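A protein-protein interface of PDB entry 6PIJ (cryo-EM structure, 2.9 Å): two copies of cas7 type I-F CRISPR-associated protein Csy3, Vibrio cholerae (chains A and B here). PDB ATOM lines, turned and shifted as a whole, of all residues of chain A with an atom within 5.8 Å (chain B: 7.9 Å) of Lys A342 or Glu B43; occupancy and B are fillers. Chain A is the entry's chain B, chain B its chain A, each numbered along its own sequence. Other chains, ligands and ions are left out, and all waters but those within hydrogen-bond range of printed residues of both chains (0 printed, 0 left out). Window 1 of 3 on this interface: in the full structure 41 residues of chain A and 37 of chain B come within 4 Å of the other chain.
OE1 of Glu B43 lies within salt-bridge range of NE of Arg A285, at 3.6 Å.
OE2 of Glu B43 is in salt-bridge range of NZ of Lys A342, at 2.6 Å.
OD1 of Asn A339 sits at hydrogen-bond distance from NH1 of Arg A285, at 3.3 Å.
The backbone carbonyl oxygen (O) of Val A283 lies within hydrogen-bond range of the side-chain amino group (NZ) of Lys A342 (2.9 Å).
The backbone carbonyl oxygen (O) of Gly A344 sits at hydrogen-bond distance from the guanidinium group (NH2) of Arg A285 (3.4 Å).
OD1 of Asn A339 sits close to O of Gly A284, at 2.9 Å.
N of Gln B41 sits close to OD1 of Asn B68, 3.1 Å away.
OE2 of Glu B43 is in hydrogen-bond range of NE2 of Gln B41 (3.2 Å).
Gly A284 touches Gln B41.
Glu B43 touches Gly A284 (OE2 to CA, 3.4 Å).
Met B42 touches Phe A286.
Phe A286 touches Ala B44 (CZ to O, 3.97 Å).
CZ of Phe A286 touches CB of Ala B48, 3.8 Å away.
CG of Phe A286 touches CD1 of Leu B64, 3.96 Å away.
Phe A306 touches Glu B43 (CZ to O, 3.6 Å).
CE1 of Phe A306 touches CB of Lys B45, 3.6 Å away.
NZ of Lys A342 touches NE2 of Gln B41 (3.8 Å).
Of chain B, only Gln B41 (3.8 Å) and Glu B43 (2.6 Å) come within 4 Å of Lys A342.
Printed residues of chain A within 4 Å of Glu B43: Gly A284, Arg A285, Phe A306 and Lys A342.
No residue of chain B comes within 4 Å of Gly A343.
Printed residues of chain A within 4 Å of Leu B64: Phe A286.
Printed residues of chain A within 4 Å of Ala B48: Phe A286 (3.8 Å).
Of the printed residues of chain A, Gln B41 touches Gly A284 and Lys A342.
Of the printed residues of chain B, Phe A286 touches Met B42 (3.2 Å), Ala B44 (3.97 Å), Ala B48 (3.8 Å) and Leu B64 (3.96 Å).
Glu A9 touches none of the printed residues of chain B.
Gly B40 touches none of the printed residues of chain A.
Of the 20 printed residues of chain A, 5 touch a printed residue of chain B.
Printed residues of chain A that touch a printed residue of chain B: Gly A284, Arg A285, Phe A286, Phe A306 and Lys A342.
Printed residues of chain B that touch a printed residue of chain A: Gln B41, Met B42, Glu B43, Ala B44, Lys B45, Ala B48 and Leu B64.
Hydrophobic or aromatic side chains of chain B that line the printed part of chain A: Ala B48 and Leu B64.
Among the printed residues, Asp or Glu carboxylates within 4 Å of a Lys or Arg side-chain nitrogen of the other chain: Arg A285 with Glu B43 and Lys A342 with Glu B43.
No position is printed for both chains.
Of the 11 pairs that touch across the chains among the printed residues, none has its exchanged pair printed and touching as well.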
ATOM      1  N   TYR A   8      35.225  20.717  -0.690  1.00  0.00           N
ATOM      2  CA  TYR A   8      35.238  21.857  -1.643  1.00  0.00           C
ATOM      3  C   TYR A   8      34.730  23.101  -0.905  1.00  0.00           C
ATOM      4  O   TYR A   8      33.920  22.946   0.030  1.00  0.00           O
ATOM      5  CB  TYR A   8      34.380  21.542  -2.872  1.00  0.00           C
ATOM      6  CG  TYR A   8      35.111  20.883  -4.015  1.00  0.00           C
ATOM      7  CD1 TYR A   8      35.287  19.508  -4.062  1.00  0.00           C
ATOM      8  CD2 TYR A   8      35.620  21.635  -5.062  1.00  0.00           C
ATOM      9  CE1 TYR A   8      35.945  18.897  -5.119  1.00  0.00           C
ATOM     10  CE2 TYR A   8      36.286  21.041  -6.123  1.00  0.00           C
ATOM     11  CZ  TYR A   8      36.452  19.667  -6.151  1.00  0.00           C
ATOM     12  OH  TYR A   8      37.106  19.076  -7.194  1.00  0.00           O
ATOM     13  N   GLU A   9      35.205  24.284  -1.302  1.00  0.00           N
ATOM     14  CA  GLU A   9      34.716  25.595  -0.793  1.00  0.00           C
ATOM     15  C   GLU A   9      33.643  26.126  -1.751  1.00  0.00           C
ATOM     16  O   GLU A   9      33.403  25.485  -2.794  1.00  0.00           O
ATOM     17  CB  GLU A   9      35.873  26.581  -0.624  1.00  0.00           C
ATOM     18  CG  GLU A   9      36.653  26.384   0.661  1.00  0.00           C
ATOM     19  CD  GLU A   9      37.538  27.558   1.039  1.00  0.00           C
ATOM     20  OE1 GLU A   9      36.994  28.598   1.465  1.00  0.00           O
ATOM     21  OE2 GLU A   9      38.765  27.438   0.886  1.00  0.00           O
ATOM     22  N   ARG A  10      33.004  27.239  -1.381  1.00  0.00           N
ATOM     23  CA  ARG A  10      31.993  27.949  -2.212  1.00  0.00           C
ATOM     24  C   ARG A  10      32.678  28.590  -3.422  1.00  0.00           C
ATOM     25  O   ARG A  10      33.850  29.002  -3.289  1.00  0.00           O
ATOM     26  CB  ARG A  10      31.268  29.032  -1.405  1.00  0.00           C
ATOM     27  CG  ARG A  10      29.892  28.623  -0.903  1.00  0.00           C
ATOM     28  CD  ARG A  10      29.217  29.737  -0.126  1.00  0.00           C
ATOM     29  NE  ARG A  10      29.552  29.692   1.293  1.00  0.00           N
ATOM     30  CZ  ARG A  10      30.534  30.365   1.897  1.00  0.00           C
ATOM     31  NH1 ARG A  10      31.331  31.183   1.223  1.00  0.00           N
ATOM     32  NH2 ARG A  10      30.716  30.215   3.199  1.00  0.00           N
ATOM     33  N   SER A  11      31.964  28.664  -4.550  1.00  0.00           N
ATOM     34  CA  SER A  11      32.329  29.473  -5.744  1.00  0.00           C
ATOM     35  C   SER A  11      31.355  30.649  -5.931  1.00  0.00           C
ATOM     36  O   SER A  11      31.746  31.602  -6.622  1.00  0.00           O
ATOM     37  CB  SER A  11      32.419  28.609  -6.976  1.00  0.00           C
ATOM     38  OG  SER A  11      33.698  28.000  -7.070  1.00  0.00           O
ATOM     39  N   TYR A 131      22.608  30.960 -13.191  1.00  0.00           N
ATOM     40  CA  TYR A 131      22.898  31.678 -11.918  1.00  0.00           C
ATOM     41  C   TYR A 131      22.551  33.166 -12.060  1.00  0.00           C
ATOM     42  O   TYR A 131      21.877  33.702 -11.159  1.00  0.00           O
ATOM     43  CB  TYR A 131      24.356  31.506 -11.481  1.00  0.00           C
ATOM     44  CG  TYR A 131      24.721  30.128 -10.986  1.00  0.00           C
ATOM     45  CD1 TYR A 131      23.992  29.506  -9.983  1.00  0.00           C
ATOM     46  CD2 TYR A 131      25.817  29.450 -11.500  1.00  0.00           C
ATOM     47  CE1 TYR A 131      24.325  28.242  -9.520  1.00  0.00           C
ATOM     48  CE2 TYR A 131      26.163  28.185 -11.049  1.00  0.00           C
ATOM     49  CZ  TYR A 131      25.416  27.579 -10.054  1.00  0.00           C
ATOM     50  OH  TYR A 131      25.755  26.336  -9.603  1.00  0.00           O
ATOM     51  N   ARG A 282      16.534  23.692  -5.449  1.00  0.00           N
ATOM     52  CA  ARG A 282      17.826  24.122  -4.850  1.00  0.00           C
ATOM     53  C   ARG A 282      18.810  22.956  -4.997  1.00  0.00           C
ATOM     54  O   ARG A 282      18.440  21.837  -4.582  1.00  0.00           O
ATOM     55  CB  ARG A 282      17.630  24.529  -3.385  1.00  0.00           C
ATOM     56  CG  ARG A 282      18.788  25.316  -2.787  1.00  0.00           C
ATOM     57  CD  ARG A 282      19.763  24.473  -1.988  1.00  0.00           C
ATOM     58  NE  ARG A 282      20.756  25.309  -1.319  1.00  0.00           N
ATOM     59  CZ  ARG A 282      21.850  25.828  -1.881  1.00  0.00           C
ATOM     60  NH1 ARG A 282      22.140  25.606  -3.154  1.00  0.00           N
ATOM     61  NH2 ARG A 282      22.665  26.575  -1.152  1.00  0.00           N
ATOM     62  N   VAL A 283      19.994  23.193  -5.578  1.00  0.00           N
ATOM     63  CA  VAL A 283      20.971  22.114  -5.931  1.00  0.00           C
ATOM     64  C   VAL A 283      21.435  21.443  -4.630  1.00  0.00           C
ATOM     65  O   VAL A 283      21.851  22.164  -3.701  1.00  0.00           O
ATOM     66  CB  VAL A 283      22.166  22.607  -6.778  1.00  0.00           C
ATOM     67  CG1 VAL A 283      21.723  23.347  -8.030  1.00  0.00           C
ATOM     68  CG2 VAL A 283      23.154  23.453  -5.989  1.00  0.00           C
ATOM     69  N   GLY A 284      21.316  20.115  -4.562  1.00  0.00           N
ATOM     70  CA  GLY A 284      21.791  19.281  -3.441  1.00  0.00           C
ATOM     71  C   GLY A 284      22.333  17.957  -3.943  1.00  0.00           C
ATOM     72  O   GLY A 284      22.539  17.830  -5.168  1.00  0.00           O
ATOM     73  N   ARG A 285      22.543  17.002  -3.035  1.00  0.00           N
ATOM     74  CA  ARG A 285      23.028  15.635  -3.363  1.00  0.00           C
ATOM     75  C   ARG A 285      21.817  14.769  -3.722  1.00  0.00           C
ATOM     76  O   ARG A 285      21.862  14.104  -4.775  1.00  0.00           O
ATOM     77  CB  ARG A 285      23.822  15.027  -2.203  1.00  0.00           C
ATOM     78  CG  ARG A 285      25.165  15.696  -1.945  1.00  0.00           C
ATOM     79  CD  ARG A 285      25.015  16.951  -1.109  1.00  0.00           C
ATOM     80  NE  ARG A 285      26.281  17.504  -0.645  1.00  0.00           N
ATOM     81  CZ  ARG A 285      26.981  18.477  -1.234  1.00  0.00           C
ATOM     82  NH1 ARG A 285      26.575  19.041  -2.364  1.00  0.00           N
ATOM     83  NH2 ARG A 285      28.112  18.879  -0.680  1.00  0.00           N
ATOM     84  N   PHE A 286      20.774  14.810  -2.888  1.00  0.00           N
ATOM     85  CA  PHE A 286      19.535  14.000  -3.021  1.00  0.00           C
ATOM     86  C   PHE A 286      18.369  14.903  -3.451  1.00  0.00           C
ATOM     87  O   PHE A 286      17.259  14.729  -2.912  1.00  0.00           O
ATOM     88  CB  PHE A 286      19.256  13.259  -1.709  1.00  0.00           C
ATOM     89  CG  PHE A 286      20.484  12.716  -1.021  1.00  0.00           C
ATOM     90  CD1 PHE A 286      21.226  11.692  -1.592  1.00  0.00           C
ATOM     91  CD2 PHE A 286      20.906  13.237   0.192  1.00  0.00           C
ATOM     92  CE1 PHE A 286      22.358  11.198  -0.961  1.00  0.00           C
ATOM     93  CE2 PHE A 286      22.039  12.741   0.823  1.00  0.00           C
ATOM     94  CZ  PHE A 286      22.762  11.723   0.245  1.00  0.00           C
ATOM     95  N   PHE A 306      26.449  11.038  -5.185  1.00  0.00           N
ATOM     96  CA  PHE A 306      27.512  10.060  -4.822  1.00  0.00           C
ATOM     97  C   PHE A 306      27.528   8.879  -5.804  1.00  0.00           C
ATOM     98  O   PHE A 306      28.582   8.222  -5.902  1.00  0.00           O
ATOM     99  CB  PHE A 306      27.348   9.597  -3.373  1.00  0.00           C
ATOM    100  CG  PHE A 306      27.382  10.718  -2.364  1.00  0.00           C
ATOM    101  CD1 PHE A 306      28.584  11.305  -1.993  1.00  0.00           C
ATOM    102  CD2 PHE A 306      26.209  11.202  -1.800  1.00  0.00           C
ATOM    103  CE1 PHE A 306      28.612  12.344  -1.074  1.00  0.00           C
ATOM    104  CE2 PHE A 306      26.240  12.239  -0.880  1.00  0.00           C
ATOM    105  CZ  PHE A 306      27.440  12.808  -0.517  1.00  0.00           C
ATOM    106  N   MET A 337      28.936  19.695 -11.732  1.00  0.00           N
ATOM    107  CA  MET A 337      29.587  21.034 -11.643  1.00  0.00           C
ATOM    108  C   MET A 337      28.782  21.944 -10.706  1.00  0.00           C
ATOM    109  O   MET A 337      29.415  22.609  -9.851  1.00  0.00           O
ATOM    110  CB  MET A 337      29.703  21.701 -13.018  1.00  0.00           C
ATOM    111  CG  MET A 337      30.708  21.043 -13.947  1.00  0.00           C
ATOM    112  SD  MET A 337      32.402  20.998 -13.306  1.00  0.00           S
ATOM    113  CE  MET A 337      32.517  19.276 -12.821  1.00  0.00           C
ATOM    114  N   ALA A 338      27.450  21.964 -10.851  1.00  0.00           N
ATOM    115  CA  ALA A 338      26.512  22.739  -9.998  1.00  0.00           C
ATOM    116  C   ALA A 338      26.723  22.388  -8.519  1.00  0.00           C
ATOM    117  O   ALA A 338      26.661  23.313  -7.683  1.00  0.00           O
ATOM    118  CB  ALA A 338      25.085  22.490 -10.423  1.00  0.00           C
ATOM    119  N   ASN A 339      26.972  21.109  -8.213  1.00  0.00           N
ATOM    120  CA  ASN A 339      27.235  20.608  -6.834  1.00  0.00           C
ATOM    121  C   ASN A 339      28.664  20.958  -6.395  1.00  0.00           C
ATOM    122  O   ASN A 339      28.844  21.177  -5.186  1.00  0.00           O
ATOM    123  CB  ASN A 339      26.975  19.104  -6.699  1.00  0.00           C
ATOM    124  CG  ASN A 339      25.554  18.778  -6.293  1.00  0.00           C
ATOM    125  OD1 ASN A 339      25.039  19.323  -5.318  1.00  0.00           O
ATOM    126  ND2 ASN A 339      24.917  17.878  -7.021  1.00  0.00           N
ATOM    127  N   LEU A 340      29.640  20.983  -7.313  1.00  0.00           N
ATOM    128  CA  LEU A 340      31.051  21.356  -7.001  1.00  0.00           C
ATOM    129  C   LEU A 340      31.154  22.864  -6.730  1.00  0.00           C
ATOM    130  O   LEU A 340      31.963  23.240  -5.855  1.00  0.00           O
ATOM    131  CB  LEU A 340      31.988  20.940  -8.144  1.00  0.00           C
ATOM    132  CG  LEU A 340      32.323  19.449  -8.261  1.00  0.00           C
ATOM    133  CD1 LEU A 340      33.539  19.249  -9.155  1.00  0.00           C
ATOM    134  CD2 LEU A 340      32.561  18.802  -6.902  1.00  0.00           C
ATOM    135  N   ILE A 341      30.381  23.690  -7.446  1.00  0.00           N
ATOM    136  CA  ILE A 341      30.300  25.173  -7.243  1.00  0.00           C
ATOM    137  C   ILE A 341      29.804  25.476  -5.818  1.00  0.00           C
ATOM    138  O   ILE A 341      30.278  26.481  -5.232  1.00  0.00           O
ATOM    139  CB  ILE A 341      29.429  25.821  -8.346  1.00  0.00           C
ATOM    140  CG1 ILE A 341      30.174  25.816  -9.684  1.00  0.00           C
ATOM    141  CG2 ILE A 341      28.966  27.225  -7.970  1.00  0.00           C
ATOM    142  CD1 ILE A 341      29.303  26.025 -10.899  1.00  0.00           C
ATOM    143  N   LYS A 342      28.916  24.630  -5.280  1.00  0.00           N
ATOM    144  CA  LYS A 342      28.276  24.782  -3.942  1.00  0.00           C
ATOM    145  C   LYS A 342      29.117  24.115  -2.846  1.00  0.00           C
ATOM    146  O   LYS A 342      29.334  24.756  -1.799  1.00  0.00           O
ATOM    147  CB  LYS A 342      26.882  24.139  -3.953  1.00  0.00           C
ATOM    148  CG  LYS A 342      26.171  24.065  -2.605  1.00  0.00           C
ATOM    149  CD  LYS A 342      24.990  23.122  -2.594  1.00  0.00           C
ATOM    150  CE  LYS A 342      24.381  22.966  -1.217  1.00  0.00           C
ATOM    151  NZ  LYS A 342      23.294  21.960  -1.211  1.00  0.00           N
ATOM    152  N   GLY A 343      29.568  22.883  -3.095  1.00  0.00           N
ATOM    153  CA  GLY A 343      29.561  21.776  -2.118  1.00  0.00           C
ATOM    154  C   GLY A 343      30.708  21.772  -1.122  1.00  0.00           C
ATOM    155  O   GLY A 343      31.227  22.852  -0.794  1.00  0.00           O
ATOM    156  N   GLY A 344      31.081  20.564  -0.679  1.00  0.00           N
ATOM    157  CA  GLY A 344      31.739  20.262   0.606  1.00  0.00           C
ATOM    158  C   GLY A 344      30.687  19.760   1.596  1.00  0.00           C
ATOM    159  O   GLY A 344      29.705  20.464   1.809  1.00  0.00           O
ATOM    160  N   MET A 345      30.825  18.559   2.183  1.00  0.00           N
ATOM    161  CA  MET A 345      31.978  17.673   2.120  1.00  0.00           C
ATOM    162  C   MET A 345      31.553  16.338   1.494  1.00  0.00           C
ATOM    163  O   MET A 345      30.480  15.828   1.878  1.00  0.00           O
ATOM    164  CB  MET A 345      32.516  17.420   3.531  1.00  0.00           C
ATOM    165  CG  MET A 345      32.750  18.691   4.324  1.00  0.00           C
ATOM    166  SD  MET A 345      33.623  18.364   5.869  1.00  0.00           S
ATOM    167  CE  MET A 345      32.261  17.895   6.932  1.00  0.00           C
ATOM    168  N   GLY B  40      20.073  23.490   7.348  1.00  0.00           N
ATOM    169  CA  GLY B  40      20.595  22.763   6.176  1.00  0.00           C
ATOM    170  C   GLY B  40      19.690  21.601   5.805  1.00  0.00           C
ATOM    171  O   GLY B  40      18.619  21.453   6.435  1.00  0.00           O
ATOM    172  N   GLN B  41      20.116  20.790   4.834  1.00  0.00           N
ATOM    173  CA  GLN B  41      19.425  19.544   4.403  1.00  0.00           C
ATOM    174  C   GLN B  41      20.391  18.365   4.575  1.00  0.00           C
ATOM    175  O   GLN B  41      21.614  18.605   4.637  1.00  0.00           O
ATOM    176  CB  GLN B  41      18.873  19.696   2.981  1.00  0.00           C
ATOM    177  CG  GLN B  41      19.933  19.902   1.903  1.00  0.00           C
ATOM    178  CD  GLN B  41      19.380  20.465   0.615  1.00  0.00           C
ATOM    179  OE1 GLN B  41      18.386  21.188   0.595  1.00  0.00           O
ATOM    180  NE2 GLN B  41      20.040  20.143  -0.485  1.00  0.00           N
ATOM    181  N   MET B  42      19.849  17.148   4.691  1.00  0.00           N
ATOM    182  CA  MET B  42      20.606  15.910   5.029  1.00  0.00           C
ATOM    183  C   MET B  42      21.470  15.532   3.819  1.00  0.00           C
ATOM    184  O   MET B  42      20.927  14.923   2.879  1.00  0.00           O
ATOM    185  CB  MET B  42      19.661  14.751   5.384  1.00  0.00           C
ATOM    186  CG  MET B  42      18.697  15.055   6.521  1.00  0.00           C
ATOM    187  SD  MET B  42      19.374  14.728   8.167  1.00  0.00           S
ATOM    188  CE  MET B  42      17.929  15.054   9.177  1.00  0.00           C
ATOM    189  N   GLU B  43      22.754  15.913   3.838  1.00  0.00           N
ATOM    190  CA  GLU B  43      23.656  15.912   2.650  1.00  0.00           C
ATOM    191  C   GLU B  43      24.864  14.979   2.824  1.00  0.00           C
ATOM    192  O   GLU B  43      25.529  14.719   1.800  1.00  0.00           O
ATOM    193  CB  GLU B  43      24.125  17.341   2.365  1.00  0.00           C
ATOM    194  CG  GLU B  43      23.096  18.172   1.620  1.00  0.00           C
ATOM    195  CD  GLU B  43      23.662  19.334   0.825  1.00  0.00           C
ATOM    196  OE1 GLU B  43      24.567  20.023   1.341  1.00  0.00           O
ATOM    197  OE2 GLU B  43      23.203  19.542  -0.315  1.00  0.00           O
ATOM    198  N   ALA B  44      25.156  14.502   4.040  1.00  0.00           N
ATOM    199  CA  ALA B  44      26.283  13.578   4.318  1.00  0.00           C
ATOM    200  C   ALA B  44      26.026  12.237   3.618  1.00  0.00           C
ATOM    201  O   ALA B  44      24.861  11.789   3.609  1.00  0.00           O
ATOM    202  CB  ALA B  44      26.474  13.402   5.806  1.00  0.00           C
ATOM    203  N   LYS B  45      27.078  11.639   3.046  1.00  0.00           N
ATOM    204  CA  LYS B  45      27.034  10.328   2.337  1.00  0.00           C
ATOM    205  C   LYS B  45      26.673   9.213   3.327  1.00  0.00           C
ATOM    206  O   LYS B  45      26.039   8.238   2.897  1.00  0.00           O
ATOM    207  CB  LYS B  45      28.377  10.022   1.667  1.00  0.00           C
ATOM    208  N   SER B  46      27.065   9.362   4.599  1.00  0.00           N
ATOM    209  CA  SER B  46      26.825   8.394   5.704  1.00  0.00           C
ATOM    210  C   SER B  46      25.322   8.180   5.951  1.00  0.00           C
ATOM    211  O   SER B  46      24.957   7.059   6.353  1.00  0.00           O
ATOM    212  CB  SER B  46      27.522   8.846   6.966  1.00  0.00           C
ATOM    213  OG  SER B  46      27.356   7.896   8.009  1.00  0.00           O
ATOM    214  N   LEU B  47      24.490   9.205   5.729  1.00  0.00           N
ATOM    215  CA  LEU B  47      23.041   9.188   6.073  1.00  0.00           C
ATOM    216  C   LEU B  47      22.239   8.374   5.046  1.00  0.00           C
ATOM    217  O   LEU B  47      21.111   7.989   5.395  1.00  0.00           O
ATOM    218  CB  LEU B  47      22.510  10.624   6.160  1.00  0.00           C
ATOM    219  CG  LEU B  47      23.233  11.554   7.136  1.00  0.00           C
ATOM    220  CD1 LEU B  47      22.582  12.928   7.152  1.00  0.00           C
ATOM    221  CD2 LEU B  47      23.275  10.972   8.542  1.00  0.00           C
ATOM    222  N   ALA B  48      22.779   8.130   3.843  1.00  0.00           N
ATOM    223  CA  ALA B  48      22.107   7.400   2.738  1.00  0.00           C
ATOM    224  C   ALA B  48      22.956   6.234   2.205  1.00  0.00           C
ATOM    225  O   ALA B  48      22.575   5.683   1.153  1.00  0.00           O
ATOM    226  CB  ALA B  48      21.778   8.372   1.633  1.00  0.00           C
ATOM    227  N   LEU B  64      15.294  11.635   4.106  1.00  0.00           N
ATOM    228  CA  LEU B  64      16.458  12.392   3.558  1.00  0.00           C
ATOM    229  C   LEU B  64      16.081  13.857   3.276  1.00  0.00           C
ATOM    230  O   LEU B  64      17.005  14.629   2.945  1.00  0.00           O
ATOM    231  CB  LEU B  64      16.976  11.702   2.286  1.00  0.00           C
ATOM    232  CG  LEU B  64      17.994  10.575   2.489  1.00  0.00           C
ATOM    233  CD1 LEU B  64      18.493  10.059   1.146  1.00  0.00           C
ATOM    234  CD2 LEU B  64      19.170  11.029   3.345  1.00  0.00           C
ATOM    235  N   GLN B  66      14.092  15.787   5.570  1.00  0.00           N
ATOM    236  CA  GLN B  66      13.884  16.497   6.863  1.00  0.00           C
ATOM    237  C   GLN B  66      15.057  17.463   7.069  1.00  0.00           C
ATOM    238  O   GLN B  66      16.203  16.981   7.106  1.00  0.00           O
ATOM    239  CB  GLN B  66      13.785  15.518   8.039  1.00  0.00           C
ATOM    240  CG  GLN B  66      12.699  14.460   7.890  1.00  0.00           C
ATOM    241  CD  GLN B  66      11.331  15.048   7.641  1.00  0.00           C
ATOM    242  OE1 GLN B  66      10.832  15.857   8.420  1.00  0.00           O
ATOM    243  NE2 GLN B  66      10.713  14.646   6.543  1.00  0.00           N
ATOM    244  N   ASN B  68      17.866  19.483   8.621  1.00  0.00           N
ATOM    245  CA  ASN B  68      18.715  19.332   9.836  1.00  0.00           C
ATOM    246  C   ASN B  68      19.199  20.716  10.271  1.00  0.00           C
ATOM    247  O   ASN B  68      19.934  21.377   9.538  1.00  0.00           O
ATOM    248  CB  ASN B  68      19.864  18.329   9.655  1.00  0.00           C
ATOM    249  CG  ASN B  68      20.808  18.638   8.512  1.00  0.00           C
ATOM    250  OD1 ASN B  68      20.426  19.279   7.538  1.00  0.00           O
ATOM    251  ND2 ASN B  68      22.041  18.170   8.615  1.00  0.00           N
